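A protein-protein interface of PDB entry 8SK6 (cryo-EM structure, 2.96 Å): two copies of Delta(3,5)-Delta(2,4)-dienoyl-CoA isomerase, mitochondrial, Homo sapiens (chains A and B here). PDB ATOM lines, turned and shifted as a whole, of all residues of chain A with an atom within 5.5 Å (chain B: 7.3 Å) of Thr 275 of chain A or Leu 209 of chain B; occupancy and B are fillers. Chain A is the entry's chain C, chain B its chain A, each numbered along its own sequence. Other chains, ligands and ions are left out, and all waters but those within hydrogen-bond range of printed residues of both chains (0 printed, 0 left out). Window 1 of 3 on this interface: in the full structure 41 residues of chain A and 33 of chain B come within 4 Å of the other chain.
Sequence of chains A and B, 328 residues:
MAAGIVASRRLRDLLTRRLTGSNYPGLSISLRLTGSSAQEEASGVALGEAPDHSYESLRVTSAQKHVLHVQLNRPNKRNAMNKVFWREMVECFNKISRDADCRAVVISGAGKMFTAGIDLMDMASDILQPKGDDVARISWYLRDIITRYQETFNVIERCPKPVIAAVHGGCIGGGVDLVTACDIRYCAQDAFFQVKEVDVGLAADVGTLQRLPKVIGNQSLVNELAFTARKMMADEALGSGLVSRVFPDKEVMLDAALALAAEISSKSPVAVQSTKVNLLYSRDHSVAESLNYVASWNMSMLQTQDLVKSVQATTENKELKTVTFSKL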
ATOM      1  N   VAL A 270     -25.874  33.114  11.719  1.00  0.00           N
ATOM      2  CA  VAL A 270     -26.165  32.771  13.110  1.00  0.00           C
ATOM      3  C   VAL A 270     -25.149  31.763  13.629  1.00  0.00           C
ATOM      4  O   VAL A 270     -24.623  31.898  14.739  1.00  0.00           O
ATOM      5  CB  VAL A 270     -27.604  32.243  13.243  1.00  0.00           C
ATOM      6  CG1 VAL A 270     -27.865  31.773  14.660  1.00  0.00           C
ATOM      7  CG2 VAL A 270     -28.598  33.317  12.849  1.00  0.00           C
ATOM      8  N   ALA A 271     -24.858  30.734  12.831  1.00  0.00           N
ATOM      9  CA  ALA A 271     -23.906  29.711  13.251  1.00  0.00           C
ATOM     10  C   ALA A 271     -22.497  30.280  13.362  1.00  0.00           C
ATOM     11  O   ALA A 271     -21.750  29.945  14.287  1.00  0.00           O
ATOM     12  CB  ALA A 271     -23.939  28.535  12.276  1.00  0.00           C
ATOM     13  N   VAL A 272     -22.112  31.140  12.416  1.00  0.00           N
ATOM     14  CA  VAL A 272     -20.767  31.712  12.431  1.00  0.00           C
ATOM     15  C   VAL A 272     -20.602  32.654  13.617  1.00  0.00           C
ATOM     16  O   VAL A 272     -19.613  32.588  14.355  1.00  0.00           O
ATOM     17  CB  VAL A 272     -20.472  32.426  11.101  1.00  0.00           C
ATOM     18  CG1 VAL A 272     -19.201  33.233  11.209  1.00  0.00           C
ATOM     19  CG2 VAL A 272     -20.353  31.417   9.981  1.00  0.00           C
ATOM     20  N   GLN A 273     -21.573  33.549  13.814  1.00  0.00           N
ATOM     21  CA  GLN A 273     -21.492  34.494  14.924  1.00  0.00           C
ATOM     22  C   GLN A 273     -21.527  33.776  16.267  1.00  0.00           C
ATOM     23  O   GLN A 273     -20.781  34.130  17.187  1.00  0.00           O
ATOM     24  CB  GLN A 273     -22.625  35.515  14.832  1.00  0.00           C
ATOM     25  CG  GLN A 273     -22.243  36.830  14.163  1.00  0.00           C
ATOM     26  CD  GLN A 273     -22.493  36.840  12.668  1.00  0.00           C
ATOM     27  OE1 GLN A 273     -23.081  37.780  12.136  1.00  0.00           O
ATOM     28  NE2 GLN A 273     -22.036  35.803  11.981  1.00  0.00           N
ATOM     29  N   SER A 274     -22.389  32.766  16.401  1.00  0.00           N
ATOM     30  CA  SER A 274     -22.462  32.020  17.652  1.00  0.00           C
ATOM     31  C   SER A 274     -21.175  31.253  17.915  1.00  0.00           C
ATOM     32  O   SER A 274     -20.774  31.076  19.070  1.00  0.00           O
ATOM     33  CB  SER A 274     -23.654  31.063  17.627  1.00  0.00           C
ATOM     34  OG  SER A 274     -24.869  31.768  17.455  1.00  0.00           O
ATOM     35  N   THR A 275     -20.518  30.782  16.853  1.00  0.00           N
ATOM     36  CA  THR A 275     -19.280  30.027  17.021  1.00  0.00           C
ATOM     37  C   THR A 275     -18.194  30.888  17.653  1.00  0.00           C
ATOM     38  O   THR A 275     -17.477  30.440  18.553  1.00  0.00           O
ATOM     39  CB  THR A 275     -18.816  29.478  15.673  1.00  0.00           C
ATOM     40  OG1 THR A 275     -19.838  28.639  15.121  1.00  0.00           O
ATOM     41  CG2 THR A 275     -17.542  28.670  15.837  1.00  0.00           C
ATOM     42  N   LYS A 276     -18.062  32.135  17.197  1.00  0.00           N
ATOM     43  CA  LYS A 276     -17.037  33.017  17.746  1.00  0.00           C
ATOM     44  C   LYS A 276     -17.318  33.344  19.208  1.00  0.00           C
ATOM     45  O   LYS A 276     -16.398  33.386  20.033  1.00  0.00           O
ATOM     46  CB  LYS A 276     -16.941  34.298  16.920  1.00  0.00           C
ATOM     47  CG  LYS A 276     -15.887  35.262  17.431  1.00  0.00           C
ATOM     48  CD  LYS A 276     -15.817  36.523  16.595  1.00  0.00           C
ATOM     49  CE  LYS A 276     -14.728  37.448  17.105  1.00  0.00           C
ATOM     50  NZ  LYS A 276     -14.596  38.661  16.255  1.00  0.00           N
ATOM     51  N   VAL A 277     -18.586  33.581  19.546  1.00  0.00           N
ATOM     52  CA  VAL A 277     -18.941  33.935  20.920  1.00  0.00           C
ATOM     53  C   VAL A 277     -18.574  32.802  21.870  1.00  0.00           C
ATOM     54  O   VAL A 277     -18.028  33.026  22.956  1.00  0.00           O
ATOM     55  CB  VAL A 277     -20.434  34.290  21.015  1.00  0.00           C
ATOM     56  CG1 VAL A 277     -20.825  34.561  22.458  1.00  0.00           C
ATOM     57  CG2 VAL A 277     -20.747  35.493  20.145  1.00  0.00           C
ATOM     58  N   ASN A 278     -18.865  31.564  21.468  1.00  0.00           N
ATOM     59  CA  ASN A 278     -18.542  30.425  22.320  1.00  0.00           C
ATOM     60  C   ASN A 278     -17.047  30.131  22.317  1.00  0.00           C
ATOM     61  O   ASN A 278     -16.501  29.668  23.324  1.00  0.00           O
ATOM     62  CB  ASN A 278     -19.338  29.200  21.876  1.00  0.00           C
ATOM     63  CG  ASN A 278     -20.829  29.392  22.035  1.00  0.00           C
ATOM     64  OD1 ASN A 278     -21.381  29.189  23.115  1.00  0.00           O
ATOM     65  ND2 ASN A 278     -21.492  29.785  20.956  1.00  0.00           N
ATOM     66  N   LEU A 279     -16.370  30.380  21.194  1.00  0.00           N
ATOM     67  CA  LEU A 279     -14.923  30.196  21.156  1.00  0.00           C
ATOM     68  C   LEU A 279     -14.218  31.182  22.078  1.00  0.00           C
ATOM     69  O   LEU A 279     -13.276  30.814  22.790  1.00  0.00           O
ATOM     70  CB  LEU A 279     -14.407  30.338  19.725  1.00  0.00           C
ATOM     71  CG  LEU A 279     -14.542  29.101  18.836  1.00  0.00           C
ATOM     72  CD1 LEU A 279     -14.102  29.409  17.416  1.00  0.00           C
ATOM     73  CD2 LEU A 279     -13.736  27.951  19.407  1.00  0.00           C
ATOM     74  N   LEU A 280     -14.655  32.442  22.076  1.00  0.00           N
ATOM     75  CA  LEU A 280     -14.071  33.428  22.979  1.00  0.00           C
ATOM     76  C   LEU A 280     -14.406  33.112  24.431  1.00  0.00           C
ATOM     77  O   LEU A 280     -13.550  33.239  25.314  1.00  0.00           O
ATOM     78  CB  LEU A 280     -14.554  34.828  22.610  1.00  0.00           C
ATOM     79  CG  LEU A 280     -14.124  35.340  21.236  1.00  0.00           C
ATOM     80  CD1 LEU A 280     -14.815  36.653  20.927  1.00  0.00           C
ATOM     81  CD2 LEU A 280     -12.617  35.497  21.177  1.00  0.00           C
ATOM     82  N   SER A 282     -15.082  30.162  25.744  1.00  0.00           N
ATOM     83  CA  SER A 282     -14.375  28.963  26.180  1.00  0.00           C
ATOM     84  C   SER A 282     -12.927  29.261  26.547  1.00  0.00           C
ATOM     85  O   SER A 282     -12.341  28.555  27.373  1.00  0.00           O
ATOM     86  CB  SER A 282     -14.433  27.894  25.091  1.00  0.00           C
ATOM     87  OG  SER A 282     -15.772  27.598  24.741  1.00  0.00           O
ATOM     88  N   ASP B 177     -15.685  15.875  18.927  1.00  0.00           N
ATOM     89  CA  ASP B 177     -15.900  15.907  20.371  1.00  0.00           C
ATOM     90  C   ASP B 177     -15.534  14.574  21.007  1.00  0.00           C
ATOM     91  O   ASP B 177     -15.069  14.530  22.152  1.00  0.00           O
ATOM     92  CB  ASP B 177     -17.353  16.256  20.679  1.00  0.00           C
ATOM     93  CG  ASP B 177     -17.873  17.389  19.829  1.00  0.00           C
ATOM     94  OD1 ASP B 177     -18.057  17.181  18.612  1.00  0.00           O
ATOM     95  OD2 ASP B 177     -18.093  18.490  20.371  1.00  0.00           O
ATOM     96  N   VAL B 195     -14.977  19.907  11.485  1.00  0.00           N
ATOM     97  CA  VAL B 195     -16.018  20.438  12.366  1.00  0.00           C
ATOM     98  C   VAL B 195     -17.191  20.806  11.460  1.00  0.00           C
ATOM     99  O   VAL B 195     -17.308  21.930  10.975  1.00  0.00           O
ATOM    100  CB  VAL B 195     -15.523  21.623  13.190  1.00  0.00           C
ATOM    101  CG1 VAL B 195     -16.599  22.080  14.159  1.00  0.00           C
ATOM    102  CG2 VAL B 195     -14.254  21.253  13.934  1.00  0.00           C
ATOM    103  N   GLU B 197     -20.281  21.228  12.105  1.00  0.00           N
ATOM    104  CA  GLU B 197     -21.442  21.828  12.755  1.00  0.00           C
ATOM    105  C   GLU B 197     -21.921  23.079  12.025  1.00  0.00           C
ATOM    106  O   GLU B 197     -23.127  23.282  11.843  1.00  0.00           O
ATOM    107  CB  GLU B 197     -21.109  22.149  14.212  1.00  0.00           C
ATOM    108  CG  GLU B 197     -20.548  20.969  14.989  1.00  0.00           C
ATOM    109  CD  GLU B 197     -21.559  19.857  15.182  1.00  0.00           C
ATOM    110  OE1 GLU B 197     -22.775  20.140  15.141  1.00  0.00           O
ATOM    111  OE2 GLU B 197     -21.139  18.698  15.374  1.00  0.00           O
ATOM    112  N   VAL B 198     -20.988  23.935  11.601  1.00  0.00           N
ATOM    113  CA  VAL B 198     -21.370  25.175  10.929  1.00  0.00           C
ATOM    114  C   VAL B 198     -22.057  24.877   9.601  1.00  0.00           C
ATOM    115  O   VAL B 198     -23.018  25.556   9.218  1.00  0.00           O
ATOM    116  CB  VAL B 198     -20.142  26.085  10.750  1.00  0.00           C
ATOM    117  CG1 VAL B 198     -20.464  27.247   9.833  1.00  0.00           C
ATOM    118  CG2 VAL B 198     -19.682  26.599  12.099  1.00  0.00           C
ATOM    119  N   LEU B 202     -25.496  25.065  12.885  1.00  0.00           N
ATOM    120  CA  LEU B 202     -25.499  25.356  14.309  1.00  0.00           C
ATOM    121  C   LEU B 202     -24.071  25.379  14.827  1.00  0.00           C
ATOM    122  O   LEU B 202     -23.176  24.738  14.271  1.00  0.00           O
ATOM    123  CB  LEU B 202     -26.319  24.328  15.102  1.00  0.00           C
ATOM    124  CG  LEU B 202     -25.772  22.899  15.159  1.00  0.00           C
ATOM    125  CD1 LEU B 202     -26.190  22.217  16.450  1.00  0.00           C
ATOM    126  CD2 LEU B 202     -26.247  22.093  13.966  1.00  0.00           C
ATOM    127  N   ALA B 203     -23.865  26.131  15.903  1.00  0.00           N
ATOM    128  CA  ALA B 203     -22.582  26.133  16.588  1.00  0.00           C
ATOM    129  C   ALA B 203     -22.399  24.829  17.347  1.00  0.00           C
ATOM    130  O   ALA B 203     -23.367  24.238  17.836  1.00  0.00           O
ATOM    131  CB  ALA B 203     -22.486  27.320  17.546  1.00  0.00           C
ATOM    132  N   ALA B 204     -21.153  24.373  17.438  1.00  0.00           N
ATOM    133  CA  ALA B 204     -20.860  23.137  18.149  1.00  0.00           C
ATOM    134  C   ALA B 204     -21.168  23.301  19.630  1.00  0.00           C
ATOM    135  O   ALA B 204     -20.515  24.083  20.328  1.00  0.00           O
ATOM    136  CB  ALA B 204     -19.399  22.747  17.945  1.00  0.00           C
ATOM    137  N   ASP B 205     -22.167  22.561  20.108  1.00  0.00           N
ATOM    138  CA  ASP B 205     -22.638  22.682  21.481  1.00  0.00           C
ATOM    139  C   ASP B 205     -22.462  21.401  22.283  1.00  0.00           C
ATOM    140  O   ASP B 205     -23.046  21.277  23.365  1.00  0.00           O
ATOM    141  CB  ASP B 205     -24.109  23.111  21.497  1.00  0.00           C
ATOM    142  CG  ASP B 205     -24.959  22.305  20.535  1.00  0.00           C
ATOM    143  OD1 ASP B 205     -24.435  21.350  19.926  1.00  0.00           O
ATOM    144  OD2 ASP B 205     -26.154  22.631  20.384  1.00  0.00           O
ATOM    145  N   VAL B 206     -21.677  20.443  21.786  1.00  0.00           N
ATOM    146  CA  VAL B 206     -21.460  19.189  22.494  1.00  0.00           C
ATOM    147  C   VAL B 206     -20.035  19.042  23.003  1.00  0.00           C
ATOM    148  O   VAL B 206     -19.734  18.060  23.695  1.00  0.00           O
ATOM    149  CB  VAL B 206     -21.841  17.983  21.612  1.00  0.00           C
ATOM    150  CG1 VAL B 206     -23.351  17.837  21.552  1.00  0.00           C
ATOM    151  CG2 VAL B 206     -21.274  18.149  20.217  1.00  0.00           C
ATOM    152  N   GLY B 207     -19.148  19.984  22.692  1.00  0.00           N
ATOM    153  CA  GLY B 207     -17.813  19.943  23.256  1.00  0.00           C
ATOM    154  C   GLY B 207     -16.685  20.362  22.335  1.00  0.00           C
ATOM    155  O   GLY B 207     -15.553  20.538  22.794  1.00  0.00           O
ATOM    156  N   THR B 208     -16.964  20.514  21.038  1.00  0.00           N
ATOM    157  CA  THR B 208     -15.909  20.895  20.102  1.00  0.00           C
ATOM    158  C   THR B 208     -15.364  22.281  20.421  1.00  0.00           C
ATOM    159  O   THR B 208     -14.153  22.462  20.579  1.00  0.00           O
ATOM    160  CB  THR B 208     -16.429  20.844  18.665  1.00  0.00           C
ATOM    161  OG1 THR B 208     -16.578  19.481  18.252  1.00  0.00           O
ATOM    162  CG2 THR B 208     -15.464  21.545  17.723  1.00  0.00           C
ATOM    163  N   LEU B 209     -16.246  23.273  20.538  1.00  0.00           N
ATOM    164  CA  LEU B 209     -15.801  24.635  20.802  1.00  0.00           C
ATOM    165  C   LEU B 209     -15.262  24.816  22.213  1.00  0.00           C
ATOM    166  O   LEU B 209     -14.668  25.862  22.499  1.00  0.00           O
ATOM    167  CB  LEU B 209     -16.943  25.621  20.562  1.00  0.00           C
ATOM    168  CG  LEU B 209     -17.534  25.639  19.153  1.00  0.00           C
ATOM    169  CD1 LEU B 209     -18.567  26.746  19.021  1.00  0.00           C
ATOM    170  CD2 LEU B 209     -16.438  25.793  18.112  1.00  0.00           C
ATOM    171  N   GLN B 210     -15.450  23.837  23.094  1.00  0.00           N
ATOM    172  CA  GLN B 210     -15.040  23.961  24.485  1.00  0.00           C
ATOM    173  C   GLN B 210     -13.738  23.241  24.797  1.00  0.00           C
ATOM    174  O   GLN B 210     -13.044  23.630  25.742  1.00  0.00           O
ATOM    175  CB  GLN B 210     -16.139  23.428  25.411  1.00  0.00           C
ATOM    176  CG  GLN B 210     -17.403  24.272  25.434  1.00  0.00           C
ATOM    177  CD  GLN B 210     -18.215  24.158  24.162  1.00  0.00           C
ATOM    178  OE1 GLN B 210     -18.172  23.139  23.476  1.00  0.00           O
ATOM    179  NE2 GLN B 210     -18.954  25.209  23.837  1.00  0.00           N
ATOM    180  N   ARG B 211     -13.386  22.210  24.035  1.00  0.00           N
ATOM    181  CA  ARG B 211     -12.177  21.437  24.288  1.00  0.00           C
ATOM    182  C   ARG B 211     -11.139  21.543  23.184  1.00  0.00           C
ATOM    183  O   ARG B 211      -9.944  21.433  23.463  1.00  0.00           O
ATOM    184  CB  ARG B 211     -12.528  19.962  24.506  1.00  0.00           C
ATOM    185  CG  ARG B 211     -13.400  19.699  25.718  1.00  0.00           C
ATOM    186  CD  ARG B 211     -13.535  18.210  25.972  1.00  0.00           C
ATOM    187  NE  ARG B 211     -14.415  17.923  27.097  1.00  0.00           N
ATOM    188  CZ  ARG B 211     -15.711  17.668  26.986  1.00  0.00           C
ATOM    189  NH1 ARG B 211     -16.313  17.656  25.809  1.00  0.00           N
ATOM    190  NH2 ARG B 211     -16.418  17.417  28.083  1.00  0.00           N
ATOM    191  N   LEU B 212     -11.557  21.745  21.935  1.00  0.00           N
ATOM    192  CA  LEU B 212     -10.588  21.859  20.848  1.00  0.00           C
ATOM    193  C   LEU B 212      -9.605  23.012  21.032  1.00  0.00           C
ATOM    194  O   LEU B 212      -8.402  22.793  20.811  1.00  0.00           O
ATOM    195  CB  LEU B 212     -11.318  21.976  19.504  1.00  0.00           C
ATOM    196  CG  LEU B 212     -10.438  22.113  18.262  1.00  0.00           C
ATOM    197  CD1 LEU B 212      -9.534  20.904  18.110  1.00  0.00           C
ATOM    198  CD2 LEU B 212     -11.293  22.304  17.022  1.00  0.00           C
ATOM    199  N   PRO B 213     -10.016  24.228  21.408  1.00  0.00           N
ATOM    200  CA  PRO B 213      -9.011  25.266  21.686  1.00  0.00           C
ATOM    201  C   PRO B 213      -8.114  24.940  22.866  1.00  0.00           C
ATOM    202  O   PRO B 213      -7.025  25.517  22.972  1.00  0.00           O
ATOM    203  CB  PRO B 213      -9.859  26.517  21.954  1.00  0.00           C
ATOM    204  CG  PRO B 213     -11.188  25.999  22.345  1.00  0.00           C
ATOM    205  CD  PRO B 213     -11.382  24.765  21.528  1.00  0.00           C
ATOM    206  N   LYS B 214      -8.529  24.037  23.752  1.00  0.00           N
ATOM    207  CA  LYS B 214      -7.756  23.701  24.939  1.00  0.00           C
ATOM    208  C   LYS B 214      -6.880  22.468  24.763  1.00  0.00           C
ATOM    209  O   LYS B 214      -6.189  22.080  25.709  1.00  0.00           O
ATOM    210  CB  LYS B 214      -8.691  23.500  26.135  1.00  0.00           C
ATOM    211  CG  LYS B 214      -9.391  24.769  26.588  1.00  0.00           C
ATOM    212  CD  LYS B 214     -10.264  24.516  27.803  1.00  0.00           C
ATOM    213  CE  LYS B 214     -10.874  25.805  28.323  1.00  0.00           C
ATOM    214  NZ  LYS B 214      -9.836  26.762  28.793  1.00  0.00           N
ATOM    215  N   VAL B 222      -7.729  26.879  14.886  1.00  0.00           N
ATOM    216  CA  VAL B 222      -9.009  26.490  15.477  1.00  0.00           C
ATOM    217  C   VAL B 222     -10.133  27.354  14.921  1.00  0.00           C
ATOM    218  O   VAL B 222     -11.201  26.853  14.549  1.00  0.00           O
ATOM    219  CB  VAL B 222      -8.942  26.577  17.011  1.00  0.00           C
ATOM    220  CG1 VAL B 222     -10.249  26.110  17.625  1.00  0.00           C
ATOM    221  CG2 VAL B 222      -7.781  25.760  17.536  1.00  0.00           C
ATOM    222  N   ASN B 223      -9.911  28.667  14.861  1.00  0.00           N
ATOM    223  CA  ASN B 223     -10.904  29.556  14.271  1.00  0.00           C
ATOM    224  C   ASN B 223     -11.096  29.256  12.791  1.00  0.00           C
ATOM    225  O   ASN B 223     -12.222  29.292  12.282  1.00  0.00           O
ATOM    226  CB  ASN B 223     -10.492  31.012  14.475  1.00  0.00           C
ATOM    227  CG  ASN B 223     -10.254  31.351  15.929  1.00  0.00           C
ATOM    228  OD1 ASN B 223     -10.873  30.774  16.821  1.00  0.00           O
ATOM    229  ND2 ASN B 223      -9.350  32.290  16.178  1.00  0.00           N
ATOM    230  N   LEU B 225     -10.701  26.367  11.260  1.00  0.00           N
ATOM    231  CA  LEU B 225     -11.446  25.121  11.112  1.00  0.00           C
ATOM    232  C   LEU B 225     -12.915  25.313  11.464  1.00  0.00           C
ATOM    233  O   LEU B 225     -13.806  24.879  10.723  1.00  0.00           O
ATOM    234  CB  LEU B 225     -10.827  24.032  11.987  1.00  0.00           C
ATOM    235  CG  LEU B 225      -9.413  23.580  11.632  1.00  0.00           C
ATOM    236  CD1 LEU B 225      -8.940  22.527  12.614  1.00  0.00           C
ATOM    237  CD2 LEU B 225      -9.366  23.051  10.212  1.00  0.00           C
ATOM    238  N   ALA B 226     -13.189  25.957  12.600  1.00  0.00           N
ATOM    239  CA  ALA B 226     -14.565  26.094  13.062  1.00  0.00           C
ATOM    240  C   ALA B 226     -15.396  26.947  12.112  1.00  0.00           C
ATOM    241  O   ALA B 226     -16.540  26.602  11.799  1.00  0.00           O
ATOM    242  CB  ALA B 226     -14.586  26.683  14.471  1.00  0.00           C
ATOM    243  N   PHE B 227     -14.837  28.060  11.636  1.00  0.00           N
ATOM    244  CA  PHE B 227     -15.601  28.994  10.819  1.00  0.00           C
ATOM    245  C   PHE B 227     -15.855  28.488   9.407  1.00  0.00           C
ATOM    246  O   PHE B 227     -16.893  28.821   8.825  1.00  0.00           O
ATOM    247  CB  PHE B 227     -14.888  30.346  10.757  1.00  0.00           C
ATOM    248  CG  PHE B 227     -14.860  31.077  12.065  1.00  0.00           C
ATOM    249  CD1 PHE B 227     -15.812  30.821  13.036  1.00  0.00           C
ATOM    250  CD2 PHE B 227     -13.887  32.022  12.324  1.00  0.00           C
ATOM    251  CE1 PHE B 227     -15.789  31.493  14.239  1.00  0.00           C
ATOM    252  CE2 PHE B 227     -13.859  32.696  13.526  1.00  0.00           C
ATOM    253  CZ  PHE B 227     -14.810  32.431  14.484  1.00  0.00           C
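NZ of Lys 214 of chain B sits close to O of Ser 282 of chain A (3.4 Å). The side-chain hydroxyl (OG) of Ser 282 of chain A is in hydrogen-bond range of the backbone carbonyl oxygen (O) of Leu 209 of chain B (3.0 Å).
O of Asn 278 of chain A sits at hydrogen-bond distance from OG of Ser 282 of chain A (2.6 Å). The side-chain hydroxyl (OG) of Ser 274 of chain A sits at hydrogen-bond distance from the backbone carbonyl oxygen (O) of Val 270 of chain A. The side-chain hydroxyl of Thr 275 of chain A lies within hydrogen-bond range of the backbone carbonyl oxygen of Ala 271 of chain A, 2.5 Å away. The side-chain amide oxygen (OE1) of Gln 210 of chain B sits close to the backbone NH (N) of Gly 207 of chain B (3.4 Å). The backbone carbonyl oxygen (O) of Glu 197 of chain B sits at hydrogen-bond distance from the backbone NH (N) of Leu 202 of chain B, 3.1 Å away.
Leu 202 of chain B touches Ala 271 of chain A. Val 272 of chain A touches Phe 227 of chain B. CB of Ala 203 of chain B touches CB of Ser 274 of chain A, at 3.9 Å. Val 198 of chain B touches Thr 275 of chain A (CG2 to OG1, 3.6 Å). CB of Ala 203 of chain B touches OG1 of Thr 275 of chain A, at 3.8 Å. Leu 209 of chain B touches Thr 275 of chain A. Phe 227 of chain B touches Lys 276 of chain A (CZ to CB, 3.7 Å). Asn 278 of chain A touches Leu 209 of chain B (CB to CD1, 3.8 Å). Leu 279 of chain A touches Leu 209 of chain B. Leu 279 of chain A touches Asn 223 of chain B (CD1 to OD1, 3.6 Å).
Thr 275 of chain A touches five residues of chain B. Of the printed residues of chain B, Asn 278 of chain A touches Leu 209. Of the printed residues of chain B, Leu 279 of chain A touches Leu 209 (3.7 Å) and Asn 223 (3.6 Å). Of the printed residues of chain A, Val 198 of chain B touches Thr 275 (3.6 Å). Thr 208 of chain B touches none of the printed residues of chain A. Of chain A, only Thr 275, Asn 278, Leu 279 and Ser 282 come within 4 Å of Leu 209 of chain B. Arg 211 of chain B touches none of the printed residues of chain A. Of the printed residues of chain A, Lys 214 of chain B touches Ser 282. The nearest residue of chain B that does not touch Thr 275 of chain A is Ala 204 of chain B (5.0 Å). The nearest printed residue of chain A that does not touch Ala 203 of chain B is Ala 271 of chain A (4.2 Å).
Printed residues of chain A that touch a printed residue of chain B: Ala 271, Val 272, Ser 274, Thr 275, Lys 276, Asn 278, Leu 279 and Ser 282. Hydrophobic or aromatic side chains of chain A within 4 Å of the printed part of chain B: Ala 271 and Leu 279. Hydrophobic or aromatic side chains of chain B that line the printed part of chain A: Val 198, Ala 203, Leu 209, Ala 226 and Phe 227. Among the printed residues, 15 pairs touch across the chains. Among the printed residues, no Asp or Glu carboxylate lies within 4 Å of a Lys or Arg side-chain nitrogen of the other chain.
No position is printed for both chains.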
